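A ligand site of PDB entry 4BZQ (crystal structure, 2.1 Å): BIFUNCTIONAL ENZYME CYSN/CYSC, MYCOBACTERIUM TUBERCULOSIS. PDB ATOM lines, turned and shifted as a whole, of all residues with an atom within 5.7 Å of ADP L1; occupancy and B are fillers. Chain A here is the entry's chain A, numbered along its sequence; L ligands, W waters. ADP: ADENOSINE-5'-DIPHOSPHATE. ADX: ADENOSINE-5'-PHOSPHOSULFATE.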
ATOM      1  N   GLY A  11     -13.426  21.657  -9.161  1.00  0.00           N
ATOM      2  CA  GLY A  11     -13.051  23.036  -9.032  1.00  0.00           C
ATOM      3  C   GLY A  11     -13.075  23.716 -10.358  1.00  0.00           C
ATOM      4  O   GLY A  11     -13.142  23.059 -11.427  1.00  0.00           O
ATOM      5  N   LEU A  12     -12.970  25.050 -10.306  1.00  0.00           N
ATOM      6  CA  LEU A  12     -12.901  25.867 -11.508  1.00  0.00           C
ATOM      7  C   LEU A  12     -11.782  25.441 -12.474  1.00  0.00           C
ATOM      8  O   LEU A  12     -10.796  24.812 -12.098  1.00  0.00           O
ATOM      9  CB  LEU A  12     -12.688  27.385 -11.137  1.00  0.00           C
ATOM     10  CG  LEU A  12     -13.799  28.023 -10.302  1.00  0.00           C
ATOM     11  CD1 LEU A  12     -13.404  29.347  -9.748  1.00  0.00           C
ATOM     12  CD2 LEU A  12     -15.006  28.219 -11.191  1.00  0.00           C
ATOM     13  N   SER A  13     -11.939  25.821 -13.730  1.00  0.00           N
ATOM     14  CA  SER A  13     -10.878  25.709 -14.666  1.00  0.00           C
ATOM     15  C   SER A  13      -9.684  26.521 -14.183  1.00  0.00           C
ATOM     16  O   SER A  13      -9.839  27.647 -13.700  1.00  0.00           O
ATOM     17  CB  SER A  13     -11.374  26.173 -16.010  1.00  0.00           C
ATOM     18  OG  SER A  13     -10.375  26.043 -16.994  1.00  0.00           O
ATOM     19  N   GLY A  14      -8.505  25.912 -14.256  1.00  0.00           N
ATOM     20  CA  GLY A  14      -7.299  26.531 -13.778  1.00  0.00           C
ATOM     21  C   GLY A  14      -7.099  26.580 -12.261  1.00  0.00           C
ATOM     22  O   GLY A  14      -6.264  27.355 -11.756  1.00  0.00           O
ATOM     23  N   SER A  15      -7.869  25.804 -11.531  1.00  0.00           N
ATOM     24  CA  SER A  15      -7.723  25.750 -10.078  1.00  0.00           C
ATOM     25  C   SER A  15      -6.621  24.769  -9.597  1.00  0.00           C
ATOM     26  O   SER A  15      -6.271  24.792  -8.408  1.00  0.00           O
ATOM     27  CB  SER A  15      -9.039  25.365  -9.473  1.00  0.00           C
ATOM     28  OG  SER A  15      -9.458  24.097  -9.967  1.00  0.00           O
ATOM     29  N   GLY A  16      -6.045  23.964 -10.493  1.00  0.00           N
ATOM     30  CA  GLY A  16      -4.921  23.061 -10.179  1.00  0.00           C
ATOM     31  C   GLY A  16      -5.278  21.584 -10.167  1.00  0.00           C
ATOM     32  O   GLY A  16      -4.514  20.757  -9.675  1.00  0.00           O
ATOM     33  N   LYS A  17      -6.434  21.242 -10.687  1.00  0.00           N
ATOM     34  CA  LYS A  17      -6.917  19.834 -10.579  1.00  0.00           C
ATOM     35  C   LYS A  17      -5.961  18.848 -11.237  1.00  0.00           C
ATOM     36  O   LYS A  17      -5.490  17.893 -10.591  1.00  0.00           O
ATOM     37  CB  LYS A  17      -8.301  19.659 -11.180  1.00  0.00           C
ATOM     38  CG  LYS A  17      -9.356  20.531 -10.542  1.00  0.00           C
ATOM     39  CD  LYS A  17     -10.717  20.328 -11.144  1.00  0.00           C
ATOM     40  CE  LYS A  17     -10.797  20.656 -12.623  1.00  0.00           C
ATOM     41  NZ  LYS A  17     -10.646  22.113 -12.827  1.00  0.00           N
ATOM     42  N   SER A  18      -5.687  19.079 -12.502  1.00  0.00           N
ATOM     43  CA  SER A  18      -4.824  18.212 -13.259  1.00  0.00           C
ATOM     44  C   SER A  18      -3.413  18.200 -12.728  1.00  0.00           C
ATOM     45  O   SER A  18      -2.775  17.164 -12.668  1.00  0.00           O
ATOM     46  CB  SER A  18      -4.748  18.646 -14.715  1.00  0.00           C
ATOM     47  OG  SER A  18      -5.909  18.271 -15.357  1.00  0.00           O
ATOM     48  N   SER A  19      -2.898  19.370 -12.355  1.00  0.00           N
ATOM     49  CA  SER A  19      -1.519  19.449 -11.829  1.00  0.00           C
ATOM     50  C   SER A  19      -1.331  18.642 -10.542  1.00  0.00           C
ATOM     51  O   SER A  19      -0.408  17.844 -10.405  1.00  0.00           O
ATOM     52  CB  SER A  19      -1.193  20.898 -11.482  1.00  0.00           C
ATOM     53  OG  SER A  19      -1.288  21.704 -12.632  1.00  0.00           O
ATOM     54  N   VAL A  20      -2.238  18.846  -9.597  1.00  0.00           N
ATOM     55  CA  VAL A  20      -2.185  18.087  -8.434  1.00  0.00           C
ATOM     56  C   VAL A  20      -2.330  16.592  -8.762  1.00  0.00           C
ATOM     57  O   VAL A  20      -1.646  15.719  -8.174  1.00  0.00           O
ATOM     58  CB  VAL A  20      -3.258  18.525  -7.442  1.00  0.00           C
ATOM     59  CG1 VAL A  20      -3.179  17.629  -6.199  1.00  0.00           C
ATOM     60  CG2 VAL A  20      -3.003  19.965  -7.023  1.00  0.00           C
ATOM     61  N   ASP A  39      -8.242  12.039 -16.794  1.00  0.00           N
ATOM     62  CA  ASP A  39      -8.375  13.486 -16.866  1.00  0.00           C
ATOM     63  C   ASP A  39      -9.526  13.881 -17.776  1.00  0.00           C
ATOM     64  O   ASP A  39      -9.585  13.413 -18.908  1.00  0.00           O
ATOM     65  CB  ASP A  39      -7.051  14.095 -17.399  1.00  0.00           C
ATOM     66  CG  ASP A  39      -7.106  15.602 -17.523  1.00  0.00           C
ATOM     67  OD1 ASP A  39      -7.876  16.110 -18.363  1.00  0.00           O
ATOM     68  OD2 ASP A  39      -6.458  16.288 -16.728  1.00  0.00           O
ATOM     69  N   PRO A  82      -9.462  14.455 -12.137  1.00  0.00           N
ATOM     70  CA  PRO A  82      -9.637  15.870 -12.215  1.00  0.00           C
ATOM     71  C   PRO A  82     -10.621  16.214 -13.300  1.00  0.00           C
ATOM     72  O   PRO A  82     -10.352  15.945 -14.501  1.00  0.00           O
ATOM     73  CB  PRO A  82      -8.270  16.388 -12.645  1.00  0.00           C
ATOM     74  CG  PRO A  82      -7.745  15.275 -13.510  1.00  0.00           C
ATOM     75  CD  PRO A  82      -8.284  14.012 -12.947  1.00  0.00           C
ATOM     76  N   THR A 112      -9.446  27.421  -5.553  1.00  0.00           N
ATOM     77  CA  THR A 112      -8.751  28.610  -5.940  1.00  0.00           C
ATOM     78  C   THR A 112      -9.815  29.615  -6.462  1.00  0.00           C
ATOM     79  O   THR A 112     -10.684  29.227  -7.229  1.00  0.00           O
ATOM     80  CB  THR A 112      -7.765  28.281  -7.051  1.00  0.00           C
ATOM     81  OG1 THR A 112      -6.812  27.324  -6.555  1.00  0.00           O
ATOM     82  CG2 THR A 112      -7.077  29.558  -7.540  1.00  0.00           C
ATOM     83  N   ARG A 120      -4.237  33.344 -13.312  1.00  0.00           N
ATOM     84  CA  ARG A 120      -3.358  32.299 -13.847  1.00  0.00           C
ATOM     85  C   ARG A 120      -3.613  32.232 -15.355  1.00  0.00           C
ATOM     86  O   ARG A 120      -2.722  32.495 -16.173  1.00  0.00           O
ATOM     87  CB  ARG A 120      -3.608  30.927 -13.223  1.00  0.00           C
ATOM     88  CG  ARG A 120      -3.482  30.831 -11.710  1.00  0.00           C
ATOM     89  CD  ARG A 120      -3.954  29.490 -11.144  1.00  0.00           C
ATOM     90  NE  ARG A 120      -3.476  29.214  -9.790  1.00  0.00           N
ATOM     91  CZ  ARG A 120      -3.953  28.288  -8.960  1.00  0.00           C
ATOM     92  NH1 ARG A 120      -4.976  27.503  -9.298  1.00  0.00           N
ATOM     93  NH2 ARG A 120      -3.423  28.126  -7.740  1.00  0.00           N
ATOM     94  N   PRO A 122      -4.098  29.678 -17.677  1.00  0.00           N
ATOM     95  CA  PRO A 122      -3.072  28.923 -18.416  1.00  0.00           C
ATOM     96  C   PRO A 122      -3.324  28.539 -19.860  1.00  0.00           C
ATOM     97  O   PRO A 122      -2.377  28.444 -20.591  1.00  0.00           O
ATOM     98  CB  PRO A 122      -2.892  27.648 -17.596  1.00  0.00           C
ATOM     99  CG  PRO A 122      -3.359  28.011 -16.233  1.00  0.00           C
ATOM    100  CD  PRO A 122      -4.466  29.006 -16.428  1.00  0.00           C
ATOM    101  N   LYS A 123      -4.564  28.288 -20.266  1.00  0.00           N
ATOM    102  CA  LYS A 123      -4.863  27.967 -21.670  1.00  0.00           C
ATOM    103  C   LYS A 123      -5.564  29.124 -22.403  1.00  0.00           C
ATOM    104  O   LYS A 123      -6.099  28.936 -23.510  1.00  0.00           O
ATOM    105  CB  LYS A 123      -5.787  26.767 -21.753  1.00  0.00           C
ATOM    106  CG  LYS A 123      -5.305  25.472 -21.107  1.00  0.00           C
ATOM    107  CD  LYS A 123      -6.476  24.764 -20.443  1.00  0.00           C
ATOM    108  CE  LYS A 123      -6.192  23.318 -20.099  1.00  0.00           C
ATOM    109  NZ  LYS A 123      -7.399  22.769 -19.452  1.00  0.00           N
ATOM    110  N   THR A 155      -5.958  24.865  -1.226  1.00  0.00           N
ATOM    111  CA  THR A 155      -6.021  26.314  -1.377  1.00  0.00           C
ATOM    112  C   THR A 155      -4.721  26.789  -1.971  1.00  0.00           C
ATOM    113  O   THR A 155      -3.724  26.122  -1.844  1.00  0.00           O
ATOM    114  CB  THR A 155      -6.293  26.991  -0.019  1.00  0.00           C
ATOM    115  OG1 THR A 155      -5.262  26.629   0.910  1.00  0.00           O
ATOM    116  CG2 THR A 155      -7.614  26.566   0.527  1.00  0.00           C
ATOM    117  N   PRO A 156      -4.704  27.995  -2.566  1.00  0.00           N
ATOM    118  CA  PRO A 156      -3.448  28.378  -3.206  1.00  0.00           C
ATOM    119  C   PRO A 156      -2.381  28.859  -2.222  1.00  0.00           C
ATOM    120  O   PRO A 156      -1.525  29.606  -2.573  1.00  0.00           O
ATOM    121  CB  PRO A 156      -3.881  29.491  -4.171  1.00  0.00           C
ATOM    122  CG  PRO A 156      -5.375  29.591  -4.071  1.00  0.00           C
ATOM    123  CD  PRO A 156      -5.745  29.001  -2.749  1.00  0.00           C
ATOM    124  N   ASP A 157      -2.415  28.384  -0.984  1.00  0.00           N
ATOM    125  CA  ASP A 157      -1.342  28.557  -0.030  1.00  0.00           C
ATOM    126  C   ASP A 157      -0.018  27.762  -0.268  1.00  0.00           C
ATOM    127  O   ASP A 157       1.027  28.146   0.289  1.00  0.00           O
ATOM    128  CB  ASP A 157      -1.876  28.088   1.326  1.00  0.00           C
ATOM    129  CG  ASP A 157      -1.957  26.546   1.424  1.00  0.00           C
ATOM    130  OD1 ASP A 157      -1.722  25.819   0.433  1.00  0.00           O
ATOM    131  OD2 ASP A 157      -2.220  26.035   2.517  1.00  0.00           O
ATOM    132  N   ARG A 158      -0.012  26.640  -0.999  1.00  0.00           N
ATOM    133  CA  ARG A 158       1.216  25.795  -1.022  1.00  0.00           C
ATOM    134  C   ARG A 158       1.670  25.476  -2.430  1.00  0.00           C
ATOM    135  O   ARG A 158       0.953  25.753  -3.367  1.00  0.00           O
ATOM    136  CB  ARG A 158       1.065  24.441  -0.324  1.00  0.00           C
ATOM    137  CG  ARG A 158       0.545  24.381   1.086  1.00  0.00           C
ATOM    138  CD  ARG A 158       0.467  22.894   1.429  1.00  0.00           C
ATOM    139  NE  ARG A 158      -0.030  22.553   2.766  1.00  0.00           N
ATOM    140  CZ  ARG A 158      -0.914  23.240   3.478  1.00  0.00           C
ATOM    141  NH1 ARG A 158      -1.433  24.364   3.036  1.00  0.00           N
ATOM    142  NH2 ARG A 158      -1.275  22.781   4.668  1.00  0.00           N
ATOM    143  N   SER A 159       2.864  24.888  -2.553  1.00  0.00           N
ATOM    144  CA  SER A 159       3.299  24.430  -3.847  1.00  0.00           C
ATOM    145  C   SER A 159       2.437  23.232  -4.278  1.00  0.00           C
ATOM    146  O   SER A 159       1.747  22.576  -3.490  1.00  0.00           O
ATOM    147  CB  SER A 159       4.802  24.067  -3.879  1.00  0.00           C
ATOM    148  OG  SER A 159       5.051  22.757  -3.485  1.00  0.00           O
ATOM    149  N   ILE A 160       2.439  22.975  -5.571  1.00  0.00           N
ATOM    150  CA  ILE A 160       1.686  21.839  -6.087  1.00  0.00           C
ATOM    151  C   ILE A 160       2.194  20.550  -5.407  1.00  0.00           C
ATOM    152  O   ILE A 160       1.390  19.729  -4.999  1.00  0.00           O
ATOM    153  CB  ILE A 160       1.779  21.813  -7.592  1.00  0.00           C
ATOM    154  CG1 ILE A 160       1.002  23.020  -8.155  1.00  0.00           C
ATOM    155  CG2 ILE A 160       1.190  20.532  -8.146  1.00  0.00           C
ATOM    156  CD1 ILE A 160       1.369  23.369  -9.576  1.00  0.00           C
ATOM    157  N   GLN A 163       0.630  20.211  -2.109  1.00  0.00           N
ATOM    158  CA  GLN A 163      -0.763  19.856  -2.256  1.00  0.00           C
ATOM    159  C   GLN A 163      -0.933  18.357  -2.564  1.00  0.00           C
ATOM    160  O   GLN A 163      -1.819  17.680  -2.010  1.00  0.00           O
ATOM    161  CB  GLN A 163      -1.420  20.731  -3.318  1.00  0.00           C
ATOM    162  CG  GLN A 163      -1.454  22.214  -2.936  1.00  0.00           C
ATOM    163  CD  GLN A 163      -2.227  23.005  -3.975  1.00  0.00           C
ATOM    164  OE1 GLN A 163      -2.156  22.691  -5.173  1.00  0.00           O
ATOM    165  NE2 GLN A 163      -2.981  23.990  -3.547  1.00  0.00           N
HETATM  166  PB  ADP L   1      -7.192  22.529 -13.854  1.00  0.00           P
HETATM  167  O1B ADP L   1      -7.706  23.308 -15.002  1.00  0.00           O
HETATM  168  O2B ADP L   1      -7.885  22.680 -12.530  1.00  0.00           O
HETATM  169  O3B ADP L   1      -6.782  21.112 -14.233  1.00  0.00           O
HETATM  170  PA  ADP L   1      -4.390  23.055 -13.917  1.00  0.00           P
HETATM  171  O1A ADP L   1      -4.293  22.826 -15.374  1.00  0.00           O
HETATM  172  O2A ADP L   1      -3.820  22.149 -12.873  1.00  0.00           O
HETATM  173  O3A ADP L   1      -5.911  23.407 -13.530  1.00  0.00           O
HETATM  174  O5' ADP L   1      -3.805  24.495 -13.866  1.00  0.00           O
HETATM  175  C5' ADP L   1      -3.707  25.213 -12.691  1.00  0.00           C
HETATM  176  C4' ADP L   1      -2.612  26.226 -12.988  1.00  0.00           C
HETATM  177  O4' ADP L   1      -2.236  26.928 -11.818  1.00  0.00           O
HETATM  178  C3' ADP L   1      -1.378  25.503 -13.434  1.00  0.00           C
HETATM  179  O3' ADP L   1      -0.761  26.242 -14.471  1.00  0.00           O
HETATM  180  C2' ADP L   1      -0.446  25.505 -12.268  1.00  0.00           C
HETATM  181  O2' ADP L   1       0.718  26.039 -12.854  1.00  0.00           O
HETATM  182  C1' ADP L   1      -0.978  26.506 -11.303  1.00  0.00           C
HETATM  183  N9  ADP L   1      -1.197  26.015  -9.934  1.00  0.00           N
HETATM  184  C8  ADP L   1      -2.167  25.192  -9.484  1.00  0.00           C
HETATM  185  N7  ADP L   1      -2.112  25.013  -8.124  1.00  0.00           N
HETATM  186  C5  ADP L   1      -1.052  25.729  -7.719  1.00  0.00           C
HETATM  187  C6  ADP L   1      -0.380  26.002  -6.436  1.00  0.00           C
HETATM  188  N6  ADP L   1      -0.851  25.418  -5.325  1.00  0.00           N
HETATM  189  N1  ADP L   1       0.684  26.821  -6.421  1.00  0.00           N
HETATM  190  C2  ADP L   1       1.163  27.386  -7.542  1.00  0.00           C
HETATM  191  N3  ADP L   1       0.598  27.175  -8.738  1.00  0.00           N
HETATM  192  C4  ADP L   1      -0.475  26.390  -8.888  1.00  0.00           C
HETATM  193  SB  ADX L   2     -16.977  19.035 -16.763  1.00  0.00           S
HETATM  194  O1B ADX L   2     -16.632  18.347 -15.510  1.00  0.00           O
HETATM  195  O2B ADX L   2     -17.894  20.123 -16.440  1.00  0.00           O
HETATM  196  O3B ADX L   2     -17.644  18.118 -17.736  1.00  0.00           O
HETATM  197  PA  ADX L   2     -14.377  18.753 -17.745  1.00  0.00           P
HETATM  198  O1A ADX L   2     -14.686  17.397 -18.302  1.00  0.00           O
HETATM  199  O2A ADX L   2     -13.492  18.776 -16.541  1.00  0.00           O
HETATM  200  O3A ADX L   2     -15.793  19.556 -17.566  1.00  0.00           O
HETATM  201  O5' ADX L   2     -13.640  19.535 -18.907  1.00  0.00           O
HETATM  202  C5' ADX L   2     -13.280  20.886 -18.663  1.00  0.00           C
HETATM  203  C4' ADX L   2     -12.046  21.293 -19.425  1.00  0.00           C
HETATM  204  O4' ADX L   2     -12.477  21.644 -20.731  1.00  0.00           O
HETATM  205  C3' ADX L   2     -11.412  22.555 -18.856  1.00  0.00           C
HETATM  206  O3' ADX L   2     -10.261  22.316 -18.033  1.00  0.00           O
HETATM  207  C2' ADX L   2     -11.096  23.375 -20.081  1.00  0.00           C
HETATM  208  O2' ADX L   2      -9.833  22.882 -20.462  1.00  0.00           O
HETATM  209  C1' ADX L   2     -11.958  22.908 -21.209  1.00  0.00           C
HETATM  210  N9  ADX L   2     -13.160  23.679 -21.554  1.00  0.00           N
HETATM  211  C8  ADX L   2     -13.519  23.937 -22.813  1.00  0.00           C
HETATM  212  N7  ADX L   2     -14.698  24.590 -22.857  1.00  0.00           N
HETATM  213  C5  ADX L   2     -15.133  24.686 -21.595  1.00  0.00           C
HETATM  214  C6  ADX L   2     -16.320  25.274 -20.960  1.00  0.00           C
HETATM  215  N6  ADX L   2     -17.218  25.851 -21.773  1.00  0.00           N
HETATM  216  N1  ADX L   2     -16.471  25.203 -19.623  1.00  0.00           N
HETATM  217  C2  ADX L   2     -15.489  24.660 -18.878  1.00  0.00           C
HETATM  218  N3  ADX L   2     -14.354  24.113 -19.395  1.00  0.00           N
HETATM  219  C4  ADX L   2     -14.150  24.088 -20.724  1.00  0.00           C
HETATM  220  O   HOH W   1     -10.502  22.204 -15.579  1.00  0.00           O
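N of Ser 19 sits at hydrogen-bond distance from O2A of ADP L1, 3.0 Å away. The side-chain hydroxyl of Ser 19 lies within hydrogen-bond range of an oxygen (O2A) of ADP L1 (2.6 Å). O of Arg 158 is in hydrogen-bond range of N6 of ADP L1. An oxygen (O2B) of ADP L1 sits at hydrogen-bond distance from the backbone NH (N) of Lys 17 (2.8 Å). The side-chain amino group (NZ) of Lys 17 lies within salt-bridge range of an oxygen (O2B) of ADP L1 (2.8 Å). An oxygen (O1B) of ADP L1 lies within hydrogen-bond range of the backbone NH of Gly 14 (2.8 Å). N of Ser 18 lies within hydrogen-bond range of O3B of ADP L1, at 2.9 Å. An oxygen (O3B) of ADP L1 sits at hydrogen-bond distance from the side-chain hydroxyl (OG) of Ser 18. A nitrogen (N6) of ADP L1 is in hydrogen-bond range of the side-chain amide oxygen of Gln 163 (3.0 Å). N of Gly 16 lies within hydrogen-bond range of O2B of ADP L1. O4' of ADP L1 sits close to NE of Arg 120. O2B of ADP L1 is in hydrogen-bond range of N of Ser 15. The side-chain hydroxyl (OG) of Ser 15 lies within hydrogen-bond range of an oxygen (O2B) of ADP L1 (3.3 Å). NZ of Lys 123 is in hydrogen-bond range of O2' of ADX L2, at 2.6 Å.
The guanidinium group (NH1) of Arg 158 lies within salt-bridge range of the side-chain carboxylate (OD1) of Asp 157, at 3.0 Å. O of Leu 12 sits at hydrogen-bond distance from NZ of Lys 17 (2.8 Å). The side-chain amino group (NZ) of Lys 17 sits at hydrogen-bond distance from the backbone carbonyl oxygen (O) of Gly 11 (3.0 Å). O of Gly 14 sits at hydrogen-bond distance from NH1 of Arg 120 (2.8 Å). The side-chain hydroxyl (OG) of Ser 18 lies within hydrogen-bond range of the side-chain carboxylate (OD2) of Asp 39, 2.5 Å away. The guanidinium group of Arg 120 is in hydrogen-bond range of the backbone carbonyl oxygen of Ser 15. The guanidinium group (NH1) of Arg 120 sits at hydrogen-bond distance from the side-chain hydroxyl (OG1) of Thr 112 (3.3 Å). O of Leu 12 lies within hydrogen-bond range of OG of Ser 15 (2.6 Å).
Leu 12 touches ADP L1 (O to O2B, 3.6 Å). Ser 13 touches ADP L1 (C to O1B, 3.9 Å). Pro 122 touches ADP L1 (CG to O3', 3.6 Å). CG1 of Ile 160 touches C5 of ADP L1, 3.4 Å away. Within 4 Å of ADP L1: Leu 12, Ser 13, Gly 14, Ser 15, Gly 16, Lys 17, Ser 18, Ser 19, Arg 120, Pro 122, Arg 158, Ile 160 and Gln 163.
Water W1 lies within hydrogen-bond range of O3' of ADX L2 (2.5 Å), NZ of Lys 17 (2.8 Å) and O1B of ADP L1 (3.1 Å).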
